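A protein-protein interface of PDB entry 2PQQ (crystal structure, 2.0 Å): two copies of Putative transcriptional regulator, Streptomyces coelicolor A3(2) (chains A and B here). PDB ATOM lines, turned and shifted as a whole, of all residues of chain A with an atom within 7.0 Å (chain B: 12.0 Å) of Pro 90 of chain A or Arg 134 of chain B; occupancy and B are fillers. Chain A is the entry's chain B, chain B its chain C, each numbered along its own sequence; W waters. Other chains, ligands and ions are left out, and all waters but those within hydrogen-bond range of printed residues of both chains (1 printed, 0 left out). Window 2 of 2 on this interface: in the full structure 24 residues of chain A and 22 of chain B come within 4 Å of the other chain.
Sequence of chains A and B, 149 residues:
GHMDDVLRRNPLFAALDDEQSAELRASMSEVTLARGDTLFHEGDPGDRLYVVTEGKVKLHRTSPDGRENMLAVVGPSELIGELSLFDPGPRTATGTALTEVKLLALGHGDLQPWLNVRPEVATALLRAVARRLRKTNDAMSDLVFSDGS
The side-chain carboxylate of Asp 87 of chain A lies within salt-bridge range of the guanidinium group of Arg 134 of chain B, at 3.0 Å. The backbone carbonyl oxygen of Pro 90 of chain A lies within hydrogen-bond range of the guanidinium group of Arg 134 of chain B, at 3.5 Å.
The backbone carbonyl oxygen of Gly 46 of chain A lies close to the side-chain hydroxyl of Ser 84 of chain A, at 3.3 Å. The backbone carbonyl oxygen (O) of Gly 89 of chain A is in hydrogen-bond range of the backbone NH (N) of Gly 46 of chain A, 2.8 Å away. The guanidinium group (NH1) of Arg 91 of chain A sits at hydrogen-bond distance from the side-chain hydroxyl (OG) of Ser 84 of chain A, at 3.2 Å.
Leu 83 of chain A touches Leu 133 of chain B (CD1 to CB, 3.6 Å). Ser 84 of chain A touches Arg 134 of chain B. Phe 86 of chain A touches Leu 126 of chain B (CB to O, 3.8 Å). Phe 86 of chain A touches Arg 127 of chain B (O to CA, 3.3 Å). Ala 130 of chain B touches Phe 86 of chain A. Asp 87 of chain A touches Arg 127 of chain B (OD1 to CG, 3.9 Å). Asp 87 of chain A touches Ala 130 of chain B. Asp 87 of chain A touches Arg 131 of chain B (OD2 to CA, 3.5 Å). Pro 88 of chain A touches Arg 127 of chain B (CD to NH2, 3.5 Å). Gly 89 of chain A touches Arg 134 of chain B (N to NH2, 3.9 Å).
Of the printed residues of chain A, Arg 134 of chain B touches Ser 84 (3.7 Å), Asp 87 (2.8 Å), Gly 89 (3.9 Å) and Pro 90 (3.5 Å). No residue of chain B comes within 4 Å of Gly 43 of chain A. No residue of chain B comes within 4 Å of Pro 45 of chain A. No residue of chain B comes within 4 Å of Gly 46 of chain A. Of chain B, only Arg 134 comes within 4 Å of Ser 84 of chain A. Asp 87 of chain A touches just these residues of chain B: Arg 127 (3.9 Å), Ala 130 (3.8 Å), Arg 131 (3.5 Å) and Arg 134 (2.8 Å). Gly 89 of chain A touches just one residue of chain B: Arg 134 (3.9 Å). No residue of chain B comes within 4 Å of Arg 91 of chain A. No residue of chain B comes within 4 Å of Thr 92 of chain A. Of the printed residues of chain A, Leu 133 of chain B touches Leu 83 (3.6 Å). Of the printed residues of chain A, Ala 130 of chain B touches Phe 86 (3.6 Å) and Asp 87 (3.8 Å). Ala 139 of chain B touches none of the printed residues of chain A. The nearest printed residue of chain A that does not touch Arg 134 of chain B is Leu 83 of chain A (4.01 Å).
Of the 18 printed residues of chain B, 6 touch a printed residue of chain A. Along chain B the printed residues that touch a printed residue of chain A span positions 126 to 134. Of the 19 printed residues of chain A, 7 touch a printed residue of chain B. Hydrophobic or aromatic side chains of chain A within 4 Å of the printed part of chain B: Leu 83, Phe 86 and Pro 88. Among the printed residues, 12 pairs touch across the chains. Among the printed residues, Asp or Glu carboxylates within 4 Å of a Lys or Arg side-chain nitrogen of the other chain: Asp 87 of chain A with Arg 134 of chain B (3.0 Å).
1 position is printed for both chains. Of the 12 pairs that touch across the chains among the printed residues, none has its exchanged pair printed and touching as well.
Water W1 lies within hydrogen-bond range of the backbone carbonyl oxygen (O) of Gly 89 of chain A, the side-chain hydroxyl (OG) of Ser 84 of chain A and the guanidinium group (NH2) of Arg 134 of chain B.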
ATOM      1  N   HIS A  41      15.949  -9.467  29.129  1.00  0.00           N
ATOM      2  CA  HIS A  41      15.811 -10.457  30.183  1.00  0.00           C
ATOM      3  C   HIS A  41      14.450 -11.137  30.083  1.00  0.00           C
ATOM      4  O   HIS A  41      13.462 -10.508  29.726  1.00  0.00           O
ATOM      5  CB  HIS A  41      15.938  -9.778  31.544  1.00  0.00           C
ATOM      6  CG  HIS A  41      17.335  -9.373  31.893  1.00  0.00           C
ATOM      7  ND1 HIS A  41      17.790  -8.076  31.772  1.00  0.00           N
ATOM      8  CD2 HIS A  41      18.378 -10.095  32.366  1.00  0.00           C
ATOM      9  CE1 HIS A  41      19.056  -8.021  32.146  1.00  0.00           C
ATOM     10  NE2 HIS A  41      19.436  -9.230  32.511  1.00  0.00           N
ATOM     11  N   GLU A  42      14.388 -12.427  30.385  1.00  0.00           N
ATOM     12  CA  GLU A  42      13.108 -13.145  30.374  1.00  0.00           C
ATOM     13  C   GLU A  42      12.140 -12.393  31.278  1.00  0.00           C
ATOM     14  O   GLU A  42      12.488 -12.063  32.402  1.00  0.00           O
ATOM     15  CB  GLU A  42      13.299 -14.578  30.896  1.00  0.00           C
ATOM     16  CG  GLU A  42      12.072 -15.490  30.733  1.00  0.00           C
ATOM     17  CD  GLU A  42      12.303 -16.924  31.234  1.00  0.00           C
ATOM     18  OE1 GLU A  42      13.419 -17.259  31.689  1.00  0.00           O
ATOM     19  OE2 GLU A  42      11.353 -17.727  31.170  1.00  0.00           O
ATOM     20  N   GLY A  43      10.926 -12.122  30.806  1.00  0.00           N
ATOM     21  CA  GLY A  43       9.959 -11.385  31.633  1.00  0.00           C
ATOM     22  C   GLY A  43       9.869  -9.894  31.331  1.00  0.00           C
ATOM     23  O   GLY A  43       8.808  -9.283  31.504  1.00  0.00           O
ATOM     24  N   ASP A  44      10.973  -9.308  30.869  1.00  0.00           N
ATOM     25  CA  ASP A  44      11.000  -7.912  30.406  1.00  0.00           C
ATOM     26  C   ASP A  44       9.828  -7.607  29.480  1.00  0.00           C
ATOM     27  O   ASP A  44       9.465  -8.437  28.675  1.00  0.00           O
ATOM     28  CB  ASP A  44      12.264  -7.637  29.591  1.00  0.00           C
ATOM     29  CG  ASP A  44      13.473  -7.378  30.437  1.00  0.00           C
ATOM     30  OD1 ASP A  44      13.397  -7.556  31.668  1.00  0.00           O
ATOM     31  OD2 ASP A  44      14.514  -6.984  29.853  1.00  0.00           O
ATOM     32  N   PRO A  45       9.250  -6.393  29.580  1.00  0.00           N
ATOM     33  CA  PRO A  45       8.272  -6.043  28.566  1.00  0.00           C
ATOM     34  C   PRO A  45       8.974  -6.059  27.202  1.00  0.00           C
ATOM     35  O   PRO A  45      10.106  -5.602  27.094  1.00  0.00           O
ATOM     36  CB  PRO A  45       7.842  -4.623  28.941  1.00  0.00           C
ATOM     37  CG  PRO A  45       8.299  -4.404  30.379  1.00  0.00           C
ATOM     38  CD  PRO A  45       9.457  -5.326  30.596  1.00  0.00           C
ATOM     39  N   GLY A  46       8.336  -6.622  26.179  1.00  0.00           N
ATOM     40  CA  GLY A  46       8.936  -6.593  24.836  1.00  0.00           C
ATOM     41  C   GLY A  46       7.979  -5.996  23.843  1.00  0.00           C
ATOM     42  O   GLY A  46       6.790  -6.327  23.873  1.00  0.00           O
ATOM     43  N   GLY A  81      12.230 -12.424  18.718  1.00  0.00           N
ATOM     44  CA  GLY A  81      11.068 -11.709  19.254  1.00  0.00           C
ATOM     45  C   GLY A  81      10.032 -11.349  18.213  1.00  0.00           C
ATOM     46  O   GLY A  81       9.395 -10.305  18.289  1.00  0.00           O
ATOM     47  N   GLU A  82       9.855 -12.224  17.230  1.00  0.00           N
ATOM     48  CA  GLU A  82       9.010 -11.921  16.093  1.00  0.00           C
ATOM     49  C   GLU A  82       7.634 -11.414  16.521  1.00  0.00           C
ATOM     50  O   GLU A  82       7.156 -10.400  16.018  1.00  0.00           O
ATOM     51  CB  GLU A  82       8.866 -13.155  15.165  1.00  0.00           C
ATOM     52  CG  GLU A  82       7.757 -12.985  14.143  1.00  0.00           C
ATOM     53  CD  GLU A  82       7.619 -14.158  13.170  1.00  0.00           C
ATOM     54  OE1 GLU A  82       8.302 -15.174  13.331  1.00  0.00           O
ATOM     55  OE2 GLU A  82       6.809 -14.044  12.247  1.00  0.00           O
ATOM     56  N   LEU A  83       6.991 -12.105  17.443  1.00  0.00           N
ATOM     57  CA  LEU A  83       5.586 -11.829  17.697  1.00  0.00           C
ATOM     58  C   LEU A  83       5.432 -10.651  18.650  1.00  0.00           C
ATOM     59  O   LEU A  83       4.341 -10.111  18.786  1.00  0.00           O
ATOM     60  CB  LEU A  83       4.858 -13.065  18.222  1.00  0.00           C
ATOM     61  CG  LEU A  83       4.827 -14.250  17.255  1.00  0.00           C
ATOM     62  CD1 LEU A  83       4.262 -15.435  17.971  1.00  0.00           C
ATOM     63  CD2 LEU A  83       4.021 -13.956  15.991  1.00  0.00           C
ATOM     64  N   SER A  84       6.548 -10.271  19.278  1.00  0.00           N
ATOM     65  CA  SER A  84       6.651  -9.071  20.112  1.00  0.00           C
ATOM     66  C   SER A  84       6.315  -7.805  19.301  1.00  0.00           C
ATOM     67  O   SER A  84       5.780  -6.840  19.836  1.00  0.00           O
ATOM     68  CB  SER A  84       8.072  -9.011  20.669  1.00  0.00           C
ATOM     69  OG  SER A  84       8.304  -7.797  21.314  1.00  0.00           O
ATOM     70  N   LEU A  85       6.591  -7.830  17.993  1.00  0.00           N
ATOM     71  CA  LEU A  85       6.239  -6.731  17.100  1.00  0.00           C
ATOM     72  C   LEU A  85       4.730  -6.505  17.032  1.00  0.00           C
ATOM     73  O   LEU A  85       4.261  -5.385  17.091  1.00  0.00           O
ATOM     74  CB  LEU A  85       6.797  -6.974  15.684  1.00  0.00           C
ATOM     75  CG  LEU A  85       6.389  -5.956  14.620  1.00  0.00           C
ATOM     76  CD1 LEU A  85       6.856  -4.526  15.003  1.00  0.00           C
ATOM     77  CD2 LEU A  85       6.959  -6.372  13.283  1.00  0.00           C
ATOM     78  N   PHE A  86       3.969  -7.590  16.945  1.00  0.00           N
ATOM     79  CA  PHE A  86       2.537  -7.525  16.738  1.00  0.00           C
ATOM     80  C   PHE A  86       1.731  -7.553  18.001  1.00  0.00           C
ATOM     81  O   PHE A  86       0.643  -6.974  18.055  1.00  0.00           O
ATOM     82  CB  PHE A  86       2.107  -8.701  15.805  1.00  0.00           C
ATOM     83  CG  PHE A  86       2.820  -8.667  14.503  1.00  0.00           C
ATOM     84  CD1 PHE A  86       2.720  -7.535  13.684  1.00  0.00           C
ATOM     85  CD2 PHE A  86       3.636  -9.727  14.114  1.00  0.00           C
ATOM     86  CE1 PHE A  86       3.415  -7.455  12.479  1.00  0.00           C
ATOM     87  CE2 PHE A  86       4.343  -9.667  12.906  1.00  0.00           C
ATOM     88  CZ  PHE A  86       4.236  -8.538  12.082  1.00  0.00           C
ATOM     89  N   ASP A  87       2.221  -8.285  18.994  1.00  0.00           N
ATOM     90  CA  ASP A  87       1.519  -8.398  20.253  1.00  0.00           C
ATOM     91  C   ASP A  87       2.525  -8.226  21.387  1.00  0.00           C
ATOM     92  O   ASP A  87       3.015  -9.193  21.959  1.00  0.00           O
ATOM     93  CB  ASP A  87       0.805  -9.741  20.352  1.00  0.00           C
ATOM     94  CG  ASP A  87       0.150  -9.939  21.678  1.00  0.00           C
ATOM     95  OD1 ASP A  87      -0.525  -8.981  22.153  1.00  0.00           O
ATOM     96  OD2 ASP A  87       0.343 -11.039  22.243  1.00  0.00           O
ATOM     97  N   PRO A  88       2.877  -6.969  21.688  1.00  0.00           N
ATOM     98  CA  PRO A  88       3.833  -6.731  22.777  1.00  0.00           C
ATOM     99  C   PRO A  88       3.471  -7.464  24.069  1.00  0.00           C
ATOM    100  O   PRO A  88       2.290  -7.540  24.419  1.00  0.00           O
ATOM    101  CB  PRO A  88       3.766  -5.205  22.946  1.00  0.00           C
ATOM    102  CG  PRO A  88       3.557  -4.713  21.527  1.00  0.00           C
ATOM    103  CD  PRO A  88       2.488  -5.711  21.015  1.00  0.00           C
ATOM    104  N   GLY A  89       4.475  -8.023  24.748  1.00  0.00           N
ATOM    105  CA  GLY A  89       4.264  -8.798  25.974  1.00  0.00           C
ATOM    106  C   GLY A  89       5.595  -9.217  26.552  1.00  0.00           C
ATOM    107  O   GLY A  89       6.632  -8.816  26.024  1.00  0.00           O
ATOM    108  N   PRO A  90       5.582 -10.011  27.646  1.00  0.00           N
ATOM    109  CA  PRO A  90       6.834 -10.430  28.281  1.00  0.00           C
ATOM    110  C   PRO A  90       7.708 -11.347  27.441  1.00  0.00           C
ATOM    111  O   PRO A  90       7.234 -12.328  26.881  1.00  0.00           O
ATOM    112  CB  PRO A  90       6.378 -11.124  29.585  1.00  0.00           C
ATOM    113  CG  PRO A  90       4.957 -11.422  29.396  1.00  0.00           C
ATOM    114  CD  PRO A  90       4.392 -10.503  28.383  1.00  0.00           C
ATOM    115  N   ARG A  91       8.986 -10.994  27.351  1.00  0.00           N
ATOM    116  CA  ARG A  91       9.994 -11.816  26.689  1.00  0.00           C
ATOM    117  C   ARG A  91       9.987 -13.249  27.232  1.00  0.00           C
ATOM    118  O   ARG A  91      10.094 -13.452  28.429  1.00  0.00           O
ATOM    119  CB  ARG A  91      11.370 -11.170  26.890  1.00  0.00           C
ATOM    120  CG  ARG A  91      11.523  -9.789  26.223  1.00  0.00           C
ATOM    121  CD  ARG A  91      11.525  -9.917  24.691  1.00  0.00           C
ATOM    122  NE  ARG A  91      11.760  -8.637  24.036  1.00  0.00           N
ATOM    123  CZ  ARG A  91      11.520  -8.379  22.750  1.00  0.00           C
ATOM    124  NH1 ARG A  91      11.017  -9.302  21.947  1.00  0.00           N
ATOM    125  NH2 ARG A  91      11.772  -7.180  22.260  1.00  0.00           N
ATOM    126  N   THR A  92       9.847 -14.243  26.352  1.00  0.00           N
ATOM    127  CA  THR A  92       9.808 -15.644  26.781  1.00  0.00           C
ATOM    128  C   THR A  92      11.184 -16.227  27.094  1.00  0.00           C
ATOM    129  O   THR A  92      11.305 -17.432  27.385  1.00  0.00           O
ATOM    130  CB  THR A  92       9.135 -16.548  25.737  1.00  0.00           C
ATOM    131  OG1 THR A  92       9.740 -16.327  24.459  1.00  0.00           O
ATOM    132  CG2 THR A  92       7.635 -16.244  25.638  1.00  0.00           C
ATOM    133  N   ALA A  93      12.226 -15.395  27.024  1.00  0.00           N
ATOM    134  CA  ALA A  93      13.594 -15.891  27.162  1.00  0.00           C
ATOM    135  C   ALA A  93      14.548 -14.744  27.388  1.00  0.00           C
ATOM    136  O   ALA A  93      14.197 -13.603  27.130  1.00  0.00           O
ATOM    137  CB  ALA A  93      14.013 -16.699  25.915  1.00  0.00           C
ATOM    138  N   PRO B  11     -12.583 -13.261  19.040  1.00  0.00           N
ATOM    139  CA  PRO B  11     -11.330 -12.564  19.367  1.00  0.00           C
ATOM    140  C   PRO B  11     -10.701 -11.745  18.202  1.00  0.00           C
ATOM    141  O   PRO B  11      -9.936 -10.793  18.455  1.00  0.00           O
ATOM    142  CB  PRO B  11     -10.402 -13.696  19.833  1.00  0.00           C
ATOM    143  CG  PRO B  11     -11.316 -14.881  20.118  1.00  0.00           C
ATOM    144  CD  PRO B  11     -12.432 -14.725  19.101  1.00  0.00           C
ATOM    145  N   LEU B  83      -8.922 -18.219   9.367  1.00  0.00           N
ATOM    146  CA  LEU B  83      -7.552 -18.084   8.906  1.00  0.00           C
ATOM    147  C   LEU B  83      -7.420 -18.091   7.368  1.00  0.00           C
ATOM    148  O   LEU B  83      -6.420 -17.600   6.816  1.00  0.00           O
ATOM    149  CB  LEU B  83      -6.683 -19.170   9.553  1.00  0.00           C
ATOM    150  CG  LEU B  83      -6.472 -18.929  11.068  1.00  0.00           C
ATOM    151  CD1 LEU B  83      -5.335 -19.784  11.562  1.00  0.00           C
ATOM    152  CD2 LEU B  83      -6.202 -17.465  11.417  1.00  0.00           C
ATOM    153  N   LEU B 125      -5.776  -6.439  13.741  1.00  0.00           N
ATOM    154  CA  LEU B 125      -5.881  -7.838  13.248  1.00  0.00           C
ATOM    155  C   LEU B 125      -4.592  -8.607  13.477  1.00  0.00           C
ATOM    156  O   LEU B 125      -4.625  -9.733  13.936  1.00  0.00           O
ATOM    157  CB  LEU B 125      -6.242  -7.866  11.774  1.00  0.00           C
ATOM    158  CG  LEU B 125      -7.536  -7.145  11.444  1.00  0.00           C
ATOM    159  CD1 LEU B 125      -7.706  -7.089   9.928  1.00  0.00           C
ATOM    160  CD2 LEU B 125      -8.688  -7.824  12.134  1.00  0.00           C
ATOM    161  N   LEU B 126      -3.451  -7.967  13.210  1.00  0.00           N
ATOM    162  CA  LEU B 126      -2.147  -8.591  13.452  1.00  0.00           C
ATOM    163  C   LEU B 126      -1.940  -8.916  14.939  1.00  0.00           C
ATOM    164  O   LEU B 126      -1.418  -9.960  15.271  1.00  0.00           O
ATOM    165  CB  LEU B 126      -1.007  -7.680  12.920  1.00  0.00           C
ATOM    166  CG  LEU B 126      -0.763  -7.755  11.392  1.00  0.00           C
ATOM    167  CD1 LEU B 126      -0.005  -6.462  10.986  1.00  0.00           C
ATOM    168  CD2 LEU B 126       0.011  -9.040  10.995  1.00  0.00           C
ATOM    169  N   ARG B 127      -2.344  -7.997  15.820  1.00  0.00           N
ATOM    170  CA  ARG B 127      -2.281  -8.209  17.266  1.00  0.00           C
ATOM    171  C   ARG B 127      -3.104  -9.435  17.627  1.00  0.00           C
ATOM    172  O   ARG B 127      -2.632 -10.312  18.337  1.00  0.00           O
ATOM    173  CB  ARG B 127      -2.801  -6.982  18.027  1.00  0.00           C
ATOM    174  CG  ARG B 127      -2.753  -7.141  19.583  1.00  0.00           C
ATOM    175  CD  ARG B 127      -3.157  -5.824  20.309  1.00  0.00           C
ATOM    176  NE  ARG B 127      -2.001  -5.344  21.045  1.00  0.00           N
ATOM    177  CZ  ARG B 127      -1.455  -4.147  20.912  1.00  0.00           C
ATOM    178  NH1 ARG B 127      -1.985  -3.258  20.085  1.00  0.00           N
ATOM    179  NH2 ARG B 127      -0.396  -3.836  21.640  1.00  0.00           N
ATOM    180  N   ALA B 128      -4.314  -9.510  17.094  1.00  0.00           N
ATOM    181  CA  ALA B 128      -5.250 -10.581  17.421  1.00  0.00           C
ATOM    182  C   ALA B 128      -4.737 -11.953  17.003  1.00  0.00           C
ATOM    183  O   ALA B 128      -4.795 -12.914  17.777  1.00  0.00           O
ATOM    184  CB  ALA B 128      -6.605 -10.295  16.759  1.00  0.00           C
ATOM    185  N   VAL B 129      -4.255 -12.067  15.774  1.00  0.00           N
ATOM    186  CA  VAL B 129      -3.637 -13.317  15.315  1.00  0.00           C
ATOM    187  C   VAL B 129      -2.390 -13.682  16.134  1.00  0.00           C
ATOM    188  O   VAL B 129      -2.241 -14.837  16.599  1.00  0.00           O
ATOM    189  CB  VAL B 129      -3.275 -13.248  13.834  1.00  0.00           C
ATOM    190  CG1 VAL B 129      -2.627 -14.571  13.386  1.00  0.00           C
ATOM    191  CG2 VAL B 129      -4.517 -12.969  13.015  1.00  0.00           C
ATOM    192  N   ALA B 130      -1.482 -12.715  16.296  1.00  0.00           N
ATOM    193  CA  ALA B 130      -0.266 -12.944  17.078  1.00  0.00           C
ATOM    194  C   ALA B 130      -0.525 -13.367  18.535  1.00  0.00           C
ATOM    195  O   ALA B 130       0.211 -14.194  19.101  1.00  0.00           O
ATOM    196  CB  ALA B 130       0.602 -11.691  17.057  1.00  0.00           C
ATOM    197  N   ARG B 131      -1.545 -12.772  19.148  1.00  0.00           N
ATOM    198  CA  ARG B 131      -1.916 -13.068  20.543  1.00  0.00           C
ATOM    199  C   ARG B 131      -2.325 -14.543  20.677  1.00  0.00           C
ATOM    200  O   ARG B 131      -1.990 -15.192  21.669  1.00  0.00           O
ATOM    201  CB  ARG B 131      -3.063 -12.153  20.963  1.00  0.00           C
ATOM    202  CG  ARG B 131      -3.565 -12.258  22.412  1.00  0.00           C
ATOM    203  CD  ARG B 131      -4.348 -10.976  22.777  1.00  0.00           C
ATOM    204  NE  ARG B 131      -5.096 -10.425  21.632  1.00  0.00           N
ATOM    205  CZ  ARG B 131      -5.590  -9.183  21.558  1.00  0.00           C
ATOM    206  NH1 ARG B 131      -5.441  -8.345  22.580  1.00  0.00           N
ATOM    207  NH2 ARG B 131      -6.245  -8.786  20.457  1.00  0.00           N
ATOM    208  N   ARG B 132      -3.040 -15.046  19.669  1.00  0.00           N
ATOM    209  CA  ARG B 132      -3.426 -16.461  19.590  1.00  0.00           C
ATOM    210  C   ARG B 132      -2.180 -17.351  19.646  1.00  0.00           C
ATOM    211  O   ARG B 132      -2.138 -18.321  20.412  1.00  0.00           O
ATOM    212  CB  ARG B 132      -4.232 -16.759  18.316  1.00  0.00           C
ATOM    213  CG  ARG B 132      -5.762 -16.745  18.478  1.00  0.00           C
ATOM    214  CD  ARG B 132      -6.329 -15.332  18.297  1.00  0.00           C
ATOM    215  NE  ARG B 132      -7.759 -15.278  17.975  1.00  0.00           N
ATOM    216  CZ  ARG B 132      -8.265 -14.799  16.832  1.00  0.00           C
ATOM    217  NH1 ARG B 132      -7.470 -14.315  15.876  1.00  0.00           N
ATOM    218  NH2 ARG B 132      -9.582 -14.804  16.636  1.00  0.00           N
ATOM    219  N   LEU B 133      -1.157 -16.987  18.889  1.00  0.00           N
ATOM    220  CA  LEU B 133       0.153 -17.593  19.013  1.00  0.00           C
ATOM    221  C   LEU B 133       0.853 -17.410  20.345  1.00  0.00           C
ATOM    222  O   LEU B 133       1.455 -18.313  20.866  1.00  0.00           O
ATOM    223  CB  LEU B 133       1.037 -17.141  17.904  1.00  0.00           C
ATOM    224  CG  LEU B 133       0.756 -17.647  16.504  1.00  0.00           C
ATOM    225  CD1 LEU B 133       1.505 -16.879  15.528  1.00  0.00           C
ATOM    226  CD2 LEU B 133       1.085 -19.084  16.401  1.00  0.00           C
ATOM    227  N   ARG B 134       0.742 -16.235  20.914  1.00  0.00           N
ATOM    228  CA  ARG B 134       1.338 -16.014  22.219  1.00  0.00           C
ATOM    229  C   ARG B 134       0.681 -16.838  23.327  1.00  0.00           C
ATOM    230  O   ARG B 134       1.385 -17.352  24.204  1.00  0.00           O
ATOM    231  CB  ARG B 134       1.364 -14.539  22.620  1.00  0.00           C
ATOM    232  CG  ARG B 134       2.076 -14.335  23.948  1.00  0.00           C
ATOM    233  CD  ARG B 134       2.139 -12.883  24.393  1.00  0.00           C
ATOM    234  NE  ARG B 134       2.927 -12.049  23.487  1.00  0.00           N
ATOM    235  CZ  ARG B 134       4.259 -12.002  23.463  1.00  0.00           C
ATOM    236  NH1 ARG B 134       4.971 -12.767  24.276  1.00  0.00           N
ATOM    237  NH2 ARG B 134       4.880 -11.201  22.606  1.00  0.00           N
ATOM    238  N   LYS B 135      -0.650 -16.933  23.334  1.00  0.00           N
ATOM    239  CA  LYS B 135      -1.286 -17.665  24.428  1.00  0.00           C
ATOM    240  C   LYS B 135      -1.112 -19.170  24.272  1.00  0.00           C
ATOM    241  O   LYS B 135      -0.967 -19.886  25.272  1.00  0.00           O
ATOM    242  CB  LYS B 135      -2.734 -17.243  24.733  1.00  0.00           C
ATOM    243  CG  LYS B 135      -3.676 -17.117  23.591  1.00  0.00           C
ATOM    244  CD  LYS B 135      -5.033 -16.566  24.082  1.00  0.00           C
ATOM    245  CE  LYS B 135      -4.997 -15.073  24.372  1.00  0.00           C
ATOM    246  NZ  LYS B 135      -5.702 -14.722  25.650  1.00  0.00           N
ATOM    247  N   THR B 136      -1.085 -19.618  23.015  1.00  0.00           N
ATOM    248  CA  THR B 136      -0.669 -20.971  22.655  1.00  0.00           C
ATOM    249  C   THR B 136       0.593 -21.368  23.408  1.00  0.00           C
ATOM    250  O   THR B 136       0.589 -22.295  24.231  1.00  0.00           O
ATOM    251  CB  THR B 136      -0.426 -21.077  21.119  1.00  0.00           C
ATOM    252  OG1 THR B 136      -1.322 -22.027  20.557  1.00  0.00           O
ATOM    253  CG2 THR B 136       0.966 -21.557  20.801  1.00  0.00           C
ATOM    254  N   ASN B 137       1.674 -20.646  23.149  1.00  0.00           N
ATOM    255  CA  ASN B 137       2.963 -21.065  23.648  1.00  0.00           C
ATOM    256  C   ASN B 137       3.161 -20.761  25.127  1.00  0.00           C
ATOM    257  O   ASN B 137       3.972 -21.411  25.783  1.00  0.00           O
ATOM    258  CB  ASN B 137       4.084 -20.534  22.748  1.00  0.00           C
ATOM    259  CG  ASN B 137       4.374 -21.460  21.571  1.00  0.00           C
ATOM    260  OD1 ASN B 137       4.658 -22.654  21.753  1.00  0.00           O
ATOM    261  ND2 ASN B 137       4.310 -20.912  20.352  1.00  0.00           N
ATOM    262  N   ASP B 138       2.380 -19.820  25.658  1.00  0.00           N
ATOM    263  CA  ASP B 138       2.317 -19.562  27.106  1.00  0.00           C
ATOM    264  C   ASP B 138       1.755 -20.772  27.877  1.00  0.00           C
ATOM    265  O   ASP B 138       1.981 -20.922  29.093  1.00  0.00           O
ATOM    266  CB  ASP B 138       1.481 -18.315  27.409  1.00  0.00           C
ATOM    267  CG  ASP B 138       2.274 -17.010  27.271  1.00  0.00           C
ATOM    268  OD1 ASP B 138       1.767 -15.981  27.767  1.00  0.00           O
ATOM    269  OD2 ASP B 138       3.380 -17.000  26.674  1.00  0.00           O
ATOM    270  N   ALA B 139       1.027 -21.622  27.154  1.00  0.00           N
ATOM    271  CA  ALA B 139       0.536 -22.893  27.675  1.00  0.00           C
ATOM    272  C   ALA B 139       1.469 -24.074  27.339  1.00  0.00           C
ATOM    273  O   ALA B 139       1.533 -25.056  28.093  1.00  0.00           O
ATOM    274  CB  ALA B 139      -0.883 -23.149  27.157  1.00  0.00           C
ATOM    275  N   MET B 140       2.181 -23.979  26.211  1.00  0.00           N
ATOM    276  CA  MET B 140       3.118 -25.032  25.774  1.00  0.00           C
ATOM    277  C   MET B 140       4.574 -24.606  26.010  1.00  0.00           C
ATOM    278  O   MET B 140       5.209 -23.981  25.144  1.00  0.00           O
ATOM    279  CB  MET B 140       2.925 -25.401  24.292  1.00  0.00           C
ATOM    280  CG  MET B 140       1.487 -25.543  23.826  1.00  0.00           C
ATOM    281  SD  MET B 140       1.314 -25.527  21.872  1.00  0.00           S
ATOM    282  CE  MET B 140      -0.596 -25.363  21.788  1.00  0.00           C
HETATM  283  O   HOH W   1       7.683  -9.740  24.017  1.00  0.00           O
